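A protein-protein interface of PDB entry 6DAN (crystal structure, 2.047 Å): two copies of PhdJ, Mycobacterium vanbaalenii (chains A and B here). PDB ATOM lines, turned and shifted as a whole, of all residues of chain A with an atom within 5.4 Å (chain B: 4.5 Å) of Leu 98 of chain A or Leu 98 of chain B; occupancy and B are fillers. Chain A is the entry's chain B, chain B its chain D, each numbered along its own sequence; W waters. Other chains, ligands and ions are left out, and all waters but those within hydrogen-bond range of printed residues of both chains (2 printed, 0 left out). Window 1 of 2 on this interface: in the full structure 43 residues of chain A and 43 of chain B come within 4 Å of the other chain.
The side-chain amide nitrogen of Asn 99 of chain B is in hydrogen-bond range of the backbone carbonyl oxygen of Ala 67 of chain A (3.0 Å).
The backbone NH (N) of Trp 125 of chain B lies within hydrogen-bond range of the side-chain hydroxyl (OH) of Tyr 301 of chain A.
The side-chain amide nitrogen (ND2) of Asn 99 of chain A is in hydrogen-bond range of the backbone carbonyl oxygen (O) of Ala 67 of chain B (3.1 Å).
OG1 of Thr 103 of chain A sits at hydrogen-bond distance from O of Asn 99 of chain A (3.0 Å).
The backbone carbonyl oxygen of Asn 99 of chain A lies within hydrogen-bond range of the side-chain hydroxyl of Thr 97 of chain A, 2.7 Å away.
The backbone carbonyl oxygen of Asn 99 of chain B sits at hydrogen-bond distance from the side-chain hydroxyl of Thr 97 of chain B.
Ala 67 of chain A touches Leu 98 of chain B (O to CB, 3.6 Å).
CB of Ala 67 of chain A touches CE3 of Trp 125 of chain B, 3.5 Å away.
CB of Thr 96 of chain A touches CH2 of Trp 125 of chain B (3.6 Å).
Ala 67 of chain B touches Leu 98 of chain A.
SD of Met 124 of chain A touches CD2 of Leu 98 of chain B (3.9 Å).
Met 124 of chain B touches Met 124 of chain A (SD to SD, 3.99 Å).
CE3 of Trp 125 of chain A touches CB of Ala 67 of chain B, at 3.6 Å.
CZ3 of Trp 125 of chain A touches CG2 of Thr 96 of chain B, 3.5 Å away.
CG of Pro 123 of chain B touches CG of Pro 300 of chain A (3.6 Å).
N of Met 124 of chain B touches OH of Tyr 301 of chain A (3.8 Å).
Printed residues of chain B within 4 Å of Ala 67 of chain A: Leu 98, Asn 99 and Trp 125.
Printed residues of chain B within 4 Å of Leu 98 of chain A: Ala 67 (3.5 Å) and Leu 98 (3.7 Å).
Of the printed residues of chain B, Met 124 of chain A touches Leu 98, Met 124 and Trp 125.
Leu 98 of chain B touches three residues of chain A.
The nearest residue of chain B that does not touch Leu 98 of chain A is Thr 96 of chain B (4.2 Å).
The nearest printed residue of chain B that does not touch Asn 99 of chain A is Leu 98 of chain B (7.2 Å).
Printed residues of chain B that touch a printed residue of chain A: Ala 67, Thr 96, Leu 98, Asn 99, Pro 123, Met 124 and Trp 125.
Hydrophobic or aromatic side chains of chain B that line the printed part of chain A: Ala 67, Leu 98, Pro 123, Met 124 and Trp 125.
Of the 13 printed residues of chain A, 9 touch a printed residue of chain B.
Among the printed residues, 17 pairs touch across the chains.
Among the printed residues, no Asp or Glu carboxylate lies within 4 Å of a Lys or Arg side-chain nitrogen of the other chain.
Ala 67 of chain A touches Asn 99 of chain B, and with the chains exchanged Asn 99 of chain A touches Ala 67 of chain B.
Thr 96 of chain A touches Trp 125 of chain B, and with the chains exchanged Trp 125 of chain A touches Thr 96 of chain B.
Met 124 of chain A touches Leu 98 of chain B, but with the chains exchanged Leu 98 of chain A does not touch Met 124 of chain B (4.2 Å).
Met 124 of chain B touches its own counterpart, Met 124 of chain A.
Positions printed for both chains: 67, 96, 97, 98, 99, 123, 124 and 125.
Of the 17 pairs that touch across the chains among the printed residues, 10 have their exchanged pair printed and touching as well.
Water W1 lies within hydrogen-bond range of N of Trp 125 of chain B (2.8 Å), O of Leu 98 of chain B (2.8 Å), OH of Tyr 301 of chain A (3.0 Å) and N of Met 124 of chain B (3.2 Å).
Water W2 bridges the backbone carbonyl oxygen of Ser 68 of chain A (2.9 Å) and the side-chain amide oxygen of Asn 99 of chain B (3.2 Å).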
ATOM      1  N   ALA A  67      -0.604 -21.490  14.037  1.00  0.00           N
ATOM      2  CA  ALA A  67      -1.326 -21.457  12.763  1.00  0.00           C
ATOM      3  C   ALA A  67      -2.669 -22.179  12.840  1.00  0.00           C
ATOM      4  O   ALA A  67      -3.666 -21.676  12.321  1.00  0.00           O
ATOM      5  CB  ALA A  67      -0.477 -22.079  11.656  1.00  0.00           C
ATOM      6  N   SER A  68      -2.717 -23.358  13.475  1.00  0.00           N
ATOM      7  CA  SER A  68      -3.829 -24.284  13.315  1.00  0.00           C
ATOM      8  C   SER A  68      -4.796 -24.335  14.489  1.00  0.00           C
ATOM      9  O   SER A  68      -5.860 -24.945  14.348  1.00  0.00           O
ATOM     10  CB  SER A  68      -3.318 -25.702  13.044  1.00  0.00           C
ATOM     11  OG  SER A  68      -2.205 -26.006  13.835  1.00  0.00           O
ATOM     12  N   THR A  96      -0.061 -14.520  16.255  1.00  0.00           N
ATOM     13  CA  THR A  96       0.371 -14.198  14.897  1.00  0.00           C
ATOM     14  C   THR A  96      -0.772 -14.504  13.947  1.00  0.00           C
ATOM     15  O   THR A  96      -1.183 -15.662  13.851  1.00  0.00           O
ATOM     16  CB  THR A  96       1.605 -15.012  14.498  1.00  0.00           C
ATOM     17  OG1 THR A  96       2.702 -14.690  15.356  1.00  0.00           O
ATOM     18  CG2 THR A  96       1.992 -14.720  13.047  1.00  0.00           C
ATOM     19  N   THR A  97      -1.289 -13.496  13.248  1.00  0.00           N
ATOM     20  CA  THR A  97      -2.347 -13.718  12.261  1.00  0.00           C
ATOM     21  C   THR A  97      -1.846 -13.348  10.863  1.00  0.00           C
ATOM     22  O   THR A  97      -0.671 -13.057  10.662  1.00  0.00           O
ATOM     23  CB  THR A  97      -3.612 -12.907  12.558  1.00  0.00           C
ATOM     24  OG1 THR A  97      -3.383 -11.533  12.195  1.00  0.00           O
ATOM     25  CG2 THR A  97      -4.009 -13.014  14.026  1.00  0.00           C
ATOM     26  N   LEU A  98      -2.776 -13.319   9.899  1.00  0.00           N
ATOM     27  CA  LEU A  98      -2.448 -12.889   8.555  1.00  0.00           C
ATOM     28  C   LEU A  98      -2.412 -11.373   8.375  1.00  0.00           C
ATOM     29  O   LEU A  98      -2.010 -10.918   7.302  1.00  0.00           O
ATOM     30  CB  LEU A  98      -3.445 -13.490   7.557  1.00  0.00           C
ATOM     31  CG  LEU A  98      -3.327 -15.002   7.444  1.00  0.00           C
ATOM     32  CD1 LEU A  98      -4.477 -15.576   6.634  1.00  0.00           C
ATOM     33  CD2 LEU A  98      -1.986 -15.288   6.787  1.00  0.00           C
ATOM     34  N   ASN A  99      -2.820 -10.573   9.353  1.00  0.00           N
ATOM     35  CA  ASN A  99      -2.787  -9.132   9.144  1.00  0.00           C
ATOM     36  C   ASN A  99      -2.669  -8.387  10.472  1.00  0.00           C
ATOM     37  O   ASN A  99      -2.816  -8.958  11.560  1.00  0.00           O
ATOM     38  CB  ASN A  99      -4.020  -8.667   8.374  1.00  0.00           C
ATOM     39  CG  ASN A  99      -5.288  -8.789   9.182  1.00  0.00           C
ATOM     40  OD1 ASN A  99      -5.573  -7.947  10.038  1.00  0.00           O
ATOM     41  ND2 ASN A  99      -6.056  -9.853   8.934  1.00  0.00           N
ATOM     42  N   THR A 100      -2.458  -7.070  10.350  1.00  0.00           N
ATOM     43  CA  THR A 100      -2.204  -6.205  11.504  1.00  0.00           C
ATOM     44  C   THR A 100      -3.422  -6.080  12.411  1.00  0.00           C
ATOM     45  O   THR A 100      -3.289  -6.086  13.642  1.00  0.00           O
ATOM     46  CB  THR A 100      -1.776  -4.822  11.013  1.00  0.00           C
ATOM     47  OG1 THR A 100      -0.695  -4.962  10.084  1.00  0.00           O
ATOM     48  CG2 THR A 100      -1.353  -3.921  12.178  1.00  0.00           C
ATOM     49  N   THR A 103      -4.252  -9.315  14.463  1.00  0.00           N
ATOM     50  CA  THR A 103      -3.235  -9.497  15.489  1.00  0.00           C
ATOM     51  C   THR A 103      -3.482  -8.560  16.662  1.00  0.00           C
ATOM     52  O   THR A 103      -3.425  -8.985  17.816  1.00  0.00           O
ATOM     53  CB  THR A 103      -1.836  -9.274  14.904  1.00  0.00           C
ATOM     54  OG1 THR A 103      -1.563 -10.263  13.892  1.00  0.00           O
ATOM     55  CG2 THR A 103      -0.783  -9.370  16.003  1.00  0.00           C
ATOM     56  N   PRO A 123       2.537 -11.064   9.468  1.00  0.00           N
ATOM     57  CA  PRO A 123       1.786 -11.618   8.326  1.00  0.00           C
ATOM     58  C   PRO A 123       2.724 -12.201   7.279  1.00  0.00           C
ATOM     59  O   PRO A 123       3.795 -11.648   7.016  1.00  0.00           O
ATOM     60  CB  PRO A 123       1.044 -10.399   7.781  1.00  0.00           C
ATOM     61  CG  PRO A 123       0.829  -9.524   9.018  1.00  0.00           C
ATOM     62  CD  PRO A 123       2.061  -9.719   9.857  1.00  0.00           C
ATOM     63  N   MET A 124       2.336 -13.331   6.672  1.00  0.00           N
ATOM     64  CA  MET A 124       3.254 -13.922   5.695  1.00  0.00           C
ATOM     65  C   MET A 124       2.644 -14.261   4.343  1.00  0.00           C
ATOM     66  O   MET A 124       3.352 -14.844   3.529  1.00  0.00           O
ATOM     67  CB  MET A 124       3.983 -15.151   6.257  1.00  0.00           C
ATOM     68  CG  MET A 124       3.167 -16.452   6.185  1.00  0.00           C
ATOM     69  SD  MET A 124       1.718 -16.351   7.306  1.00  0.00           S
ATOM     70  CE  MET A 124       2.423 -17.082   8.748  1.00  0.00           C
ATOM     71  N   TRP A 125       1.394 -13.867   4.048  1.00  0.00           N
ATOM     72  CA  TRP A 125       0.860 -14.143   2.713  1.00  0.00           C
ATOM     73  C   TRP A 125       1.750 -13.519   1.642  1.00  0.00           C
ATOM     74  O   TRP A 125       2.204 -14.205   0.712  1.00  0.00           O
ATOM     75  CB  TRP A 125      -0.579 -13.643   2.580  1.00  0.00           C
ATOM     76  CG  TRP A 125      -1.316 -14.053   1.304  1.00  0.00           C
ATOM     77  CD1 TRP A 125      -0.879 -13.927   0.008  1.00  0.00           C
ATOM     78  CD2 TRP A 125      -2.631 -14.627   1.222  1.00  0.00           C
ATOM     79  NE1 TRP A 125      -1.844 -14.388  -0.869  1.00  0.00           N
ATOM     80  CE2 TRP A 125      -2.922 -14.829  -0.146  1.00  0.00           C
ATOM     81  CE3 TRP A 125      -3.586 -14.999   2.173  1.00  0.00           C
ATOM     82  CZ2 TRP A 125      -4.135 -15.377  -0.580  1.00  0.00           C
ATOM     83  CZ3 TRP A 125      -4.781 -15.538   1.737  1.00  0.00           C
ATOM     84  CH2 TRP A 125      -5.041 -15.724   0.374  1.00  0.00           C
ATOM     85  N   PRO A 300      -3.867 -28.306   9.149  1.00  0.00           N
ATOM     86  CA  PRO A 300      -3.563 -29.256   8.079  1.00  0.00           C
ATOM     87  C   PRO A 300      -2.221 -29.978   8.181  1.00  0.00           C
ATOM     88  O   PRO A 300      -1.874 -30.668   7.226  1.00  0.00           O
ATOM     89  CB  PRO A 300      -3.542 -28.353   6.854  1.00  0.00           C
ATOM     90  CG  PRO A 300      -2.850 -27.107   7.384  1.00  0.00           C
ATOM     91  CD  PRO A 300      -3.262 -26.989   8.859  1.00  0.00           C
ATOM     92  N   TYR A 301      -1.485 -29.834   9.281  1.00  0.00           N
ATOM     93  CA  TYR A 301      -0.100 -30.313   9.338  1.00  0.00           C
ATOM     94  C   TYR A 301      -0.023 -31.687  10.000  1.00  0.00           C
ATOM     95  O   TYR A 301       0.582 -31.878  11.057  1.00  0.00           O
ATOM     96  CB  TYR A 301       0.781 -29.286  10.051  1.00  0.00           C
ATOM     97  CG  TYR A 301       0.787 -27.977   9.307  1.00  0.00           C
ATOM     98  CD1 TYR A 301       1.315 -27.906   8.025  1.00  0.00           C
ATOM     99  CD2 TYR A 301       0.204 -26.834   9.842  1.00  0.00           C
ATOM    100  CE1 TYR A 301       1.306 -26.730   7.314  1.00  0.00           C
ATOM    101  CE2 TYR A 301       0.197 -25.634   9.131  1.00  0.00           C
ATOM    102  CZ  TYR A 301       0.750 -25.601   7.861  1.00  0.00           C
ATOM    103  OH  TYR A 301       0.752 -24.444   7.118  1.00  0.00           O
ATOM    104  N   ALA B  67      -5.877 -11.698   2.702  1.00  0.00           N
ATOM    105  CA  ALA B  67      -5.050 -11.809   3.900  1.00  0.00           C
ATOM    106  C   ALA B  67      -5.427 -10.760   4.941  1.00  0.00           C
ATOM    107  O   ALA B  67      -5.524 -11.067   6.133  1.00  0.00           O
ATOM    108  CB  ALA B  67      -3.571 -11.691   3.527  1.00  0.00           C
ATOM    109  N   THR B  96      -9.460 -18.146   2.440  1.00  0.00           N
ATOM    110  CA  THR B  96      -8.160 -18.748   2.702  1.00  0.00           C
ATOM    111  C   THR B  96      -7.715 -18.314   4.089  1.00  0.00           C
ATOM    112  O   THR B  96      -7.617 -17.111   4.352  1.00  0.00           O
ATOM    113  CB  THR B  96      -7.133 -18.315   1.652  1.00  0.00           C
ATOM    114  OG1 THR B  96      -7.527 -18.802   0.364  1.00  0.00           O
ATOM    115  CG2 THR B  96      -5.762 -18.848   1.997  1.00  0.00           C
ATOM    116  N   THR B  97      -7.447 -19.280   4.973  1.00  0.00           N
ATOM    117  CA  THR B  97      -6.962 -18.952   6.312  1.00  0.00           C
ATOM    118  C   THR B  97      -5.675 -19.700   6.613  1.00  0.00           C
ATOM    119  O   THR B  97      -5.082 -20.324   5.721  1.00  0.00           O
ATOM    120  CB  THR B  97      -8.005 -19.288   7.369  1.00  0.00           C
ATOM    121  OG1 THR B  97      -8.067 -20.715   7.541  1.00  0.00           O
ATOM    122  CG2 THR B  97      -9.364 -18.766   6.931  1.00  0.00           C
ATOM    123  N   LEU B  98      -5.230 -19.666   7.859  1.00  0.00           N
ATOM    124  CA  LEU B  98      -4.016 -20.383   8.217  1.00  0.00           C
ATOM    125  C   LEU B  98      -4.261 -21.853   8.563  1.00  0.00           C
ATOM    126  O   LEU B  98      -3.296 -22.578   8.815  1.00  0.00           O
ATOM    127  CB  LEU B  98      -3.309 -19.675   9.383  1.00  0.00           C
ATOM    128  CG  LEU B  98      -2.542 -18.381   9.058  1.00  0.00           C
ATOM    129  CD1 LEU B  98      -2.158 -17.626  10.358  1.00  0.00           C
ATOM    130  CD2 LEU B  98      -1.305 -18.667   8.196  1.00  0.00           C
ATOM    131  N   ASN B  99      -5.505 -22.330   8.573  1.00  0.00           N
ATOM    132  CA  ASN B  99      -5.725 -23.731   8.923  1.00  0.00           C
ATOM    133  C   ASN B  99      -7.044 -24.235   8.336  1.00  0.00           C
ATOM    134  O   ASN B  99      -7.899 -23.458   7.905  1.00  0.00           O
ATOM    135  CB  ASN B  99      -5.685 -23.924  10.446  1.00  0.00           C
ATOM    136  CG  ASN B  99      -6.843 -23.260  11.153  1.00  0.00           C
ATOM    137  OD1 ASN B  99      -7.988 -23.711  11.054  1.00  0.00           O
ATOM    138  ND2 ASN B  99      -6.557 -22.185  11.871  1.00  0.00           N
ATOM    139  N   PRO B 123      -3.302 -23.192   3.768  1.00  0.00           N
ATOM    140  CA  PRO B 123      -2.446 -22.667   4.839  1.00  0.00           C
ATOM    141  C   PRO B 123      -0.983 -22.684   4.430  1.00  0.00           C
ATOM    142  O   PRO B 123      -0.510 -23.613   3.759  1.00  0.00           O
ATOM    143  CB  PRO B 123      -2.719 -23.620   6.009  1.00  0.00           C
ATOM    144  CG  PRO B 123      -4.085 -24.123   5.763  1.00  0.00           C
ATOM    145  CD  PRO B 123      -4.239 -24.215   4.266  1.00  0.00           C
ATOM    146  N   MET B 124      -0.264 -21.629   4.822  1.00  0.00           N
ATOM    147  CA  MET B 124       1.122 -21.479   4.394  1.00  0.00           C
ATOM    148  C   MET B 124       2.110 -21.121   5.508  1.00  0.00           C
ATOM    149  O   MET B 124       3.258 -20.791   5.196  1.00  0.00           O
ATOM    150  CB  MET B 124       1.200 -20.439   3.265  1.00  0.00           C
ATOM    151  CG  MET B 124       1.199 -18.988   3.693  1.00  0.00           C
ATOM    152  SD  MET B 124      -0.283 -18.488   4.597  1.00  0.00           S
ATOM    153  CE  MET B 124      -1.527 -18.589   3.284  1.00  0.00           C
ATOM    154  N   TRP B 125       1.734 -21.204   6.797  1.00  0.00           N
ATOM    155  CA  TRP B 125       2.737 -20.968   7.847  1.00  0.00           C
ATOM    156  C   TRP B 125       3.945 -21.880   7.657  1.00  0.00           C
ATOM    157  O   TRP B 125       5.096 -21.422   7.632  1.00  0.00           O
ATOM    158  CB  TRP B 125       2.137 -21.179   9.236  1.00  0.00           C
ATOM    159  CG  TRP B 125       3.058 -20.745  10.356  1.00  0.00           C
ATOM    160  CD1 TRP B 125       4.385 -21.088  10.530  1.00  0.00           C
ATOM    161  CD2 TRP B 125       2.717 -19.907  11.470  1.00  0.00           C
ATOM    162  NE1 TRP B 125       4.877 -20.492  11.670  1.00  0.00           N
ATOM    163  CE2 TRP B 125       3.875 -19.769  12.264  1.00  0.00           C
ATOM    164  CE3 TRP B 125       1.549 -19.239  11.856  1.00  0.00           C
ATOM    165  CZ2 TRP B 125       3.894 -19.003  13.425  1.00  0.00           C
ATOM    166  CZ3 TRP B 125       1.568 -18.491  13.020  1.00  0.00           C
ATOM    167  CH2 TRP B 125       2.729 -18.369  13.782  1.00  0.00           C
HETATM  168  O   HOH W   1      -0.692 -21.932   7.979  1.00  0.00           O
HETATM  169  O   HOH W   2      -7.088 -26.543  12.253  1.00  0.00           O
